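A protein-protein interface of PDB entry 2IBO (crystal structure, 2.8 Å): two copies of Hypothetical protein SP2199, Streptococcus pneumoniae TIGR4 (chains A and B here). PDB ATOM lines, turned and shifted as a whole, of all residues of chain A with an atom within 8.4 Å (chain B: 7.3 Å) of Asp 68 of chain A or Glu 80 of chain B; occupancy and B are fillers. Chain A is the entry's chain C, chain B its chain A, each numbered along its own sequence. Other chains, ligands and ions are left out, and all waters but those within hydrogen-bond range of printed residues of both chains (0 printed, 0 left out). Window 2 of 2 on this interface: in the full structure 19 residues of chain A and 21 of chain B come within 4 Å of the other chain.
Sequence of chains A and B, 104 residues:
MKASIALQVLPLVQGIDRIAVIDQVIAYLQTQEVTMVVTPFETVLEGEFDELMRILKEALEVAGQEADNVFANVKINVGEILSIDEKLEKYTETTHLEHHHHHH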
ATOM      1  N   PRO A  11       1.274 -23.254 -13.638  1.00  0.00           N
ATOM      2  CA  PRO A  11       2.145 -23.151 -14.823  1.00  0.00           C
ATOM      3  C   PRO A  11       2.655 -21.714 -14.883  1.00  0.00           C
ATOM      4  O   PRO A  11       1.878 -20.782 -14.678  1.00  0.00           O
ATOM      5  CB  PRO A  11       1.201 -23.473 -15.980  1.00  0.00           C
ATOM      6  CG  PRO A  11       0.122 -24.310 -15.327  1.00  0.00           C
ATOM      7  CD  PRO A  11      -0.106 -23.577 -14.033  1.00  0.00           C
ATOM      8  N   LEU A  12       3.940 -21.523 -15.164  1.00  0.00           N
ATOM      9  CA  LEU A  12       4.499 -20.170 -15.184  1.00  0.00           C
ATOM     10  C   LEU A  12       5.230 -19.764 -16.474  1.00  0.00           C
ATOM     11  O   LEU A  12       6.277 -19.111 -16.409  1.00  0.00           O
ATOM     12  CB  LEU A  12       5.461 -20.009 -13.997  1.00  0.00           C
ATOM     13  CG  LEU A  12       5.139 -20.710 -12.667  1.00  0.00           C
ATOM     14  CD1 LEU A  12       6.371 -20.670 -11.779  1.00  0.00           C
ATOM     15  CD2 LEU A  12       3.951 -20.054 -11.966  1.00  0.00           C
ATOM     16  N   VAL A  13       4.690 -20.121 -17.638  1.00  0.00           N
ATOM     17  CA  VAL A  13       5.355 -19.766 -18.894  1.00  0.00           C
ATOM     18  C   VAL A  13       4.592 -18.757 -19.775  1.00  0.00           C
ATOM     19  O   VAL A  13       5.162 -17.737 -20.186  1.00  0.00           O
ATOM     20  CB  VAL A  13       5.665 -21.034 -19.759  1.00  0.00           C
ATOM     21  CG1 VAL A  13       6.685 -20.690 -20.848  1.00  0.00           C
ATOM     22  CG2 VAL A  13       6.186 -22.166 -18.879  1.00  0.00           C
ATOM     23  N   GLN A  14       3.325 -19.048 -20.053  1.00  0.00           N
ATOM     24  CA  GLN A  14       2.526 -18.216 -20.946  1.00  0.00           C
ATOM     25  C   GLN A  14       1.581 -17.313 -20.160  1.00  0.00           C
ATOM     26  O   GLN A  14       2.006 -16.583 -19.266  1.00  0.00           O
ATOM     27  CB  GLN A  14       1.733 -19.087 -21.922  1.00  0.00           C
ATOM     28  CG  GLN A  14       2.035 -18.812 -23.385  1.00  0.00           C
ATOM     29  CD  GLN A  14       3.465 -19.147 -23.759  1.00  0.00           C
ATOM     30  OE1 GLN A  14       3.931 -18.785 -24.839  1.00  0.00           O
ATOM     31  NE2 GLN A  14       4.165 -19.840 -22.867  1.00  0.00           N
ATOM     32  N   ASP A  17      -3.449 -19.604 -21.756  1.00  0.00           N
ATOM     33  CA  ASP A  17      -2.761 -20.889 -21.745  1.00  0.00           C
ATOM     34  C   ASP A  17      -2.931 -21.593 -20.404  1.00  0.00           C
ATOM     35  O   ASP A  17      -3.088 -22.813 -20.348  1.00  0.00           O
ATOM     36  CB  ASP A  17      -1.275 -20.704 -22.058  1.00  0.00           C
ATOM     37  CG  ASP A  17      -0.849 -21.432 -23.318  1.00  0.00           C
ATOM     38  OD1 ASP A  17      -0.061 -22.395 -23.213  1.00  0.00           O
ATOM     39  OD2 ASP A  17      -1.252 -21.113 -24.457  1.00  0.00           O
ATOM     40  N   VAL A  21      -3.791 -25.474 -19.307  1.00  0.00           N
ATOM     41  CA  VAL A  21      -3.007 -26.571 -18.756  1.00  0.00           C
ATOM     42  C   VAL A  21      -3.641 -27.076 -17.478  1.00  0.00           C
ATOM     43  O   VAL A  21      -3.570 -28.264 -17.164  1.00  0.00           O
ATOM     44  CB  VAL A  21      -1.574 -26.136 -18.472  1.00  0.00           C
ATOM     45  CG1 VAL A  21      -1.541 -24.654 -18.216  1.00  0.00           C
ATOM     46  CG2 VAL A  21      -1.020 -26.896 -17.269  1.00  0.00           C
ATOM     47  N   ALA A  63       0.684 -31.997 -17.052  1.00  0.00           N
ATOM     48  CA  ALA A  63       0.918 -30.559 -16.970  1.00  0.00           C
ATOM     49  C   ALA A  63       2.253 -30.173 -17.573  1.00  0.00           C
ATOM     50  O   ALA A  63       2.357 -29.146 -18.242  1.00  0.00           O
ATOM     51  CB  ALA A  63       0.862 -30.103 -15.524  1.00  0.00           C
ATOM     52  N   GLY A  64       3.267 -31.002 -17.333  1.00  0.00           N
ATOM     53  CA  GLY A  64       4.606 -30.732 -17.832  1.00  0.00           C
ATOM     54  C   GLY A  64       4.744 -30.822 -19.337  1.00  0.00           C
ATOM     55  O   GLY A  64       5.712 -30.322 -19.917  1.00  0.00           O
ATOM     56  N   GLN A  65       3.786 -31.474 -19.980  1.00  0.00           N
ATOM     57  CA  GLN A  65       3.827 -31.593 -21.427  1.00  0.00           C
ATOM     58  C   GLN A  65       2.782 -30.639 -21.989  1.00  0.00           C
ATOM     59  O   GLN A  65       1.989 -31.004 -22.849  1.00  0.00           O
ATOM     60  CB  GLN A  65       3.520 -33.030 -21.851  1.00  0.00           C
ATOM     61  CG  GLN A  65       3.877 -33.325 -23.297  1.00  0.00           C
ATOM     62  CD  GLN A  65       3.557 -34.751 -23.695  1.00  0.00           C
ATOM     63  OE1 GLN A  65       4.001 -35.705 -23.050  1.00  0.00           O
ATOM     64  NE2 GLN A  65       2.786 -34.905 -24.767  1.00  0.00           N
ATOM     65  N   GLU A  66       2.790 -29.415 -21.474  1.00  0.00           N
ATOM     66  CA  GLU A  66       1.850 -28.376 -21.884  1.00  0.00           C
ATOM     67  C   GLU A  66       2.466 -27.026 -21.508  1.00  0.00           C
ATOM     68  O   GLU A  66       1.985 -25.966 -21.912  1.00  0.00           O
ATOM     69  CB  GLU A  66       0.518 -28.558 -21.154  1.00  0.00           C
ATOM     70  CG  GLU A  66      -0.667 -27.922 -21.859  1.00  0.00           C
ATOM     71  CD  GLU A  66      -1.354 -28.873 -22.823  1.00  0.00           C
ATOM     72  OE1 GLU A  66      -2.142 -28.392 -23.665  1.00  0.00           O
ATOM     73  OE2 GLU A  66      -1.120 -30.099 -22.732  1.00  0.00           O
ATOM     74  N   ALA A  67       3.535 -27.092 -20.716  1.00  0.00           N
ATOM     75  CA  ALA A  67       4.267 -25.919 -20.262  1.00  0.00           C
ATOM     76  C   ALA A  67       5.678 -26.378 -19.941  1.00  0.00           C
ATOM     77  O   ALA A  67       5.877 -27.531 -19.577  1.00  0.00           O
ATOM     78  CB  ALA A  67       3.610 -25.339 -19.024  1.00  0.00           C
ATOM     79  N   ASP A  68       6.657 -25.490 -20.075  1.00  0.00           N
ATOM     80  CA  ASP A  68       8.042 -25.858 -19.788  1.00  0.00           C
ATOM     81  C   ASP A  68       8.384 -25.725 -18.311  1.00  0.00           C
ATOM     82  O   ASP A  68       9.304 -26.376 -17.816  1.00  0.00           O
ATOM     83  CB  ASP A  68       9.007 -25.011 -20.624  1.00  0.00           C
ATOM     84  CG  ASP A  68       9.167 -25.541 -22.032  1.00  0.00           C
ATOM     85  OD1 ASP A  68       8.155 -25.597 -22.763  1.00  0.00           O
ATOM     86  OD2 ASP A  68      10.301 -25.909 -22.407  1.00  0.00           O
ATOM     87  N   ASN A  69       7.639 -24.876 -17.615  1.00  0.00           N
ATOM     88  CA  ASN A  69       7.847 -24.652 -16.194  1.00  0.00           C
ATOM     89  C   ASN A  69       6.569 -24.898 -15.420  1.00  0.00           C
ATOM     90  O   ASN A  69       5.624 -24.121 -15.496  1.00  0.00           O
ATOM     91  CB  ASN A  69       8.331 -23.227 -15.947  1.00  0.00           C
ATOM     92  CG  ASN A  69       9.828 -23.149 -15.796  1.00  0.00           C
ATOM     93  OD1 ASN A  69      10.381 -23.592 -14.788  1.00  0.00           O
ATOM     94  ND2 ASN A  69      10.501 -22.592 -16.802  1.00  0.00           N
ATOM     95  N   VAL A  70       6.545 -25.987 -14.667  1.00  0.00           N
ATOM     96  CA  VAL A  70       5.370 -26.314 -13.881  1.00  0.00           C
ATOM     97  C   VAL A  70       5.689 -26.386 -12.396  1.00  0.00           C
ATOM     98  O   VAL A  70       6.641 -27.048 -11.980  1.00  0.00           O
ATOM     99  CB  VAL A  70       4.765 -27.656 -14.335  1.00  0.00           C
ATOM    100  CG1 VAL A  70       3.510 -27.961 -13.541  1.00  0.00           C
ATOM    101  CG2 VAL A  70       4.443 -27.598 -15.822  1.00  0.00           C
ATOM    102  N   PHE A  71       4.910 -25.667 -11.599  1.00  0.00           N
ATOM    103  CA  PHE A  71       5.096 -25.691 -10.157  1.00  0.00           C
ATOM    104  C   PHE A  71       3.812 -26.208  -9.542  1.00  0.00           C
ATOM    105  O   PHE A  71       2.718 -25.855  -9.984  1.00  0.00           O
ATOM    106  CB  PHE A  71       5.411 -24.299  -9.590  1.00  0.00           C
ATOM    107  CG  PHE A  71       5.560 -24.300  -8.096  1.00  0.00           C
ATOM    108  CD1 PHE A  71       4.434 -24.242  -7.272  1.00  0.00           C
ATOM    109  CD2 PHE A  71       6.810 -24.469  -7.506  1.00  0.00           C
ATOM    110  CE1 PHE A  71       4.547 -24.366  -5.886  1.00  0.00           C
ATOM    111  CE2 PHE A  71       6.932 -24.594  -6.119  1.00  0.00           C
ATOM    112  CZ  PHE A  71       5.796 -24.544  -5.310  1.00  0.00           C
ATOM    113  N   MET B   1      11.779 -34.869 -17.101  1.00  0.00           N
ATOM    114  CA  MET B   1      13.125 -35.149 -16.529  1.00  0.00           C
ATOM    115  C   MET B   1      13.408 -34.367 -15.245  1.00  0.00           C
ATOM    116  O   MET B   1      12.927 -34.743 -14.181  1.00  0.00           O
ATOM    117  CB  MET B   1      14.209 -34.841 -17.561  1.00  0.00           C
ATOM    118  CG  MET B   1      15.628 -35.096 -17.072  1.00  0.00           C
ATOM    119  SD  MET B   1      16.926 -34.690 -18.448  1.00  0.00           S
ATOM    120  CE  MET B   1      16.598 -32.760 -18.583  1.00  0.00           C
ATOM    121  N   LYS B   2      14.183 -33.286 -15.344  1.00  0.00           N
ATOM    122  CA  LYS B   2      14.545 -32.488 -14.171  1.00  0.00           C
ATOM    123  C   LYS B   2      13.370 -32.136 -13.274  1.00  0.00           C
ATOM    124  O   LYS B   2      12.305 -31.721 -13.753  1.00  0.00           O
ATOM    125  CB  LYS B   2      15.267 -31.206 -14.588  1.00  0.00           C
ATOM    126  CG  LYS B   2      16.775 -31.353 -14.695  1.00  0.00           C
ATOM    127  CD  LYS B   2      17.436 -30.076 -15.207  1.00  0.00           C
ATOM    128  CE  LYS B   2      17.028 -29.788 -16.657  1.00  0.00           C
ATOM    129  NZ  LYS B   2      17.664 -28.564 -17.231  1.00  0.00           N
ATOM    130  N   ASN B  77       8.432 -29.076  -8.567  1.00  0.00           N
ATOM    131  CA  ASN B  77       8.816 -28.143  -9.617  1.00  0.00           C
ATOM    132  C   ASN B  77       9.387 -29.023 -10.729  1.00  0.00           C
ATOM    133  O   ASN B  77      10.436 -29.641 -10.559  1.00  0.00           O
ATOM    134  CB  ASN B  77       9.863 -27.154  -9.080  1.00  0.00           C
ATOM    135  CG  ASN B  77      10.286 -26.122 -10.105  1.00  0.00           C
ATOM    136  OD1 ASN B  77       9.536 -25.798 -11.023  1.00  0.00           O
ATOM    137  ND2 ASN B  77      11.482 -25.582  -9.941  1.00  0.00           N
ATOM    138  N   VAL B  78       8.671 -29.099 -11.850  1.00  0.00           N
ATOM    139  CA  VAL B  78       9.082 -29.924 -12.987  1.00  0.00           C
ATOM    140  C   VAL B  78       9.252 -29.164 -14.293  1.00  0.00           C
ATOM    141  O   VAL B  78       8.631 -28.117 -14.501  1.00  0.00           O
ATOM    142  CB  VAL B  78       8.068 -31.070 -13.263  1.00  0.00           C
ATOM    143  CG1 VAL B  78       8.214 -32.140 -12.220  1.00  0.00           C
ATOM    144  CG2 VAL B  78       6.619 -30.522 -13.288  1.00  0.00           C
ATOM    145  N   GLY B  79      10.084 -29.730 -15.170  1.00  0.00           N
ATOM    146  CA  GLY B  79      10.352 -29.139 -16.466  1.00  0.00           C
ATOM    147  C   GLY B  79      11.720 -28.494 -16.508  1.00  0.00           C
ATOM    148  O   GLY B  79      12.628 -28.909 -15.784  1.00  0.00           O
ATOM    149  N   GLU B  80      11.881 -27.485 -17.362  1.00  0.00           N
ATOM    150  CA  GLU B  80      13.159 -26.788 -17.464  1.00  0.00           C
ATOM    151  C   GLU B  80      13.254 -25.850 -16.276  1.00  0.00           C
ATOM    152  O   GLU B  80      13.034 -24.647 -16.394  1.00  0.00           O
ATOM    153  CB  GLU B  80      13.254 -26.015 -18.779  1.00  0.00           C
ATOM    154  CG  GLU B  80      13.559 -26.892 -19.992  1.00  0.00           C
ATOM    155  CD  GLU B  80      14.834 -27.722 -19.826  1.00  0.00           C
ATOM    156  OE1 GLU B  80      14.787 -28.779 -19.152  1.00  0.00           O
ATOM    157  OE2 GLU B  80      15.888 -27.314 -20.364  1.00  0.00           O
ATOM    158  N   ILE B  81      13.583 -26.441 -15.131  1.00  0.00           N
ATOM    159  CA  ILE B  81      13.694 -25.743 -13.859  1.00  0.00           C
ATOM    160  C   ILE B  81      15.131 -25.377 -13.517  1.00  0.00           C
ATOM    161  O   ILE B  81      16.065 -26.063 -13.928  1.00  0.00           O
ATOM    162  CB  ILE B  81      13.100 -26.624 -12.730  1.00  0.00           C
ATOM    163  CG1 ILE B  81      13.789 -27.999 -12.673  1.00  0.00           C
ATOM    164  CG2 ILE B  81      11.652 -26.945 -13.046  1.00  0.00           C
ATOM    165  CD1 ILE B  81      14.976 -28.094 -11.763  1.00  0.00           C
ATOM    166  N   LEU B  82      15.306 -24.288 -12.778  1.00  0.00           N
ATOM    167  CA  LEU B  82      16.635 -23.858 -12.368  1.00  0.00           C
ATOM    168  C   LEU B  82      17.025 -24.779 -11.219  1.00  0.00           C
ATOM    169  O   LEU B  82      16.150 -25.276 -10.500  1.00  0.00           O
ATOM    170  CB  LEU B  82      16.612 -22.404 -11.891  1.00  0.00           C
ATOM    171  CG  LEU B  82      16.129 -21.356 -12.896  1.00  0.00           C
ATOM    172  CD1 LEU B  82      14.647 -21.552 -13.170  1.00  0.00           C
ATOM    173  CD2 LEU B  82      16.369 -19.962 -12.340  1.00  0.00           C
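The backbone carbonyl oxygen (O) of Lys 2 of chain B lies within hydrogen-bond range of the backbone NH (N) of Gly 79 of chain B (3.3 Å).
NZ of Lys 2 of chain B is in salt-bridge range of OE1 of Glu 80 of chain B.
N of Leu 12 of chain A lies within hydrogen-bond range of O of Asn 69 of chain A, 3.1 Å away.
The backbone carbonyl oxygen (O) of Val 70 of chain A sits close to the side-chain amide oxygen (OD1) of Asn 77 of chain B, at 3.3 Å.
The backbone NH (N) of Val 78 of chain B lies within hydrogen-bond range of the backbone carbonyl oxygen (O) of Val 70 of chain A (2.9 Å).
The backbone NH of Glu 80 of chain B lies within hydrogen-bond range of the backbone carbonyl oxygen of Asp 68 of chain A, at 2.8 Å.
O of Glu 80 of chain B sits close to OD1 of Asn 69 of chain A (3.3 Å).
Asp 68 of chain A touches Val 78 of chain B (O to O, 3.8 Å).
Asp 68 of chain A touches Gly 79 of chain B (O to CA, 3.2 Å).
C of Asn 69 of chain A touches O of Val 78 of chain B, 3.9 Å away.
CG2 of Ile 81 of chain B touches OD1 of Asn 69 of chain A (3.99 Å).
Asp 68 of chain A touches just these residues of chain B: Val 78, Gly 79 and Glu 80.
Gly 79 of chain B touches just one residue of chain A: Asp 68 (3.2 Å).
Printed residues of chain B within 4 Å of Val 70 of chain A: Asn 77 (3.3 Å) and Val 78 (2.9 Å).
Printed residues of chain A within 4 Å of Val 78 of chain B: Asp 68, Asn 69 and Val 70.
Of the printed residues of chain A, Asn 77 of chain B touches Val 70.
Met 1 of chain B touches none of the printed residues of chain A.
The nearest printed residue of chain B that does not touch Asn 69 of chain A is Asn 77 of chain B (4.4 Å).
No position is printed for both chains.
Of the 8 pairs that touch across the chains among the printed residues, none has its exchanged pair printed and touching as well.
Hydrophobic or aromatic side chains of chain B within 4 Å of the printed part of chain A: Val 78 and Ile 81.
Of the 15 printed residues of chain A, 3 touch a printed residue of chain B.
Hydrophobic or aromatic side chains of chain A that line the printed part of chain B: Val 70.
Among the printed residues, no Asp or Glu carboxylate lies within 4 Å of a Lys or Arg side-chain nitrogen of the other chain.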
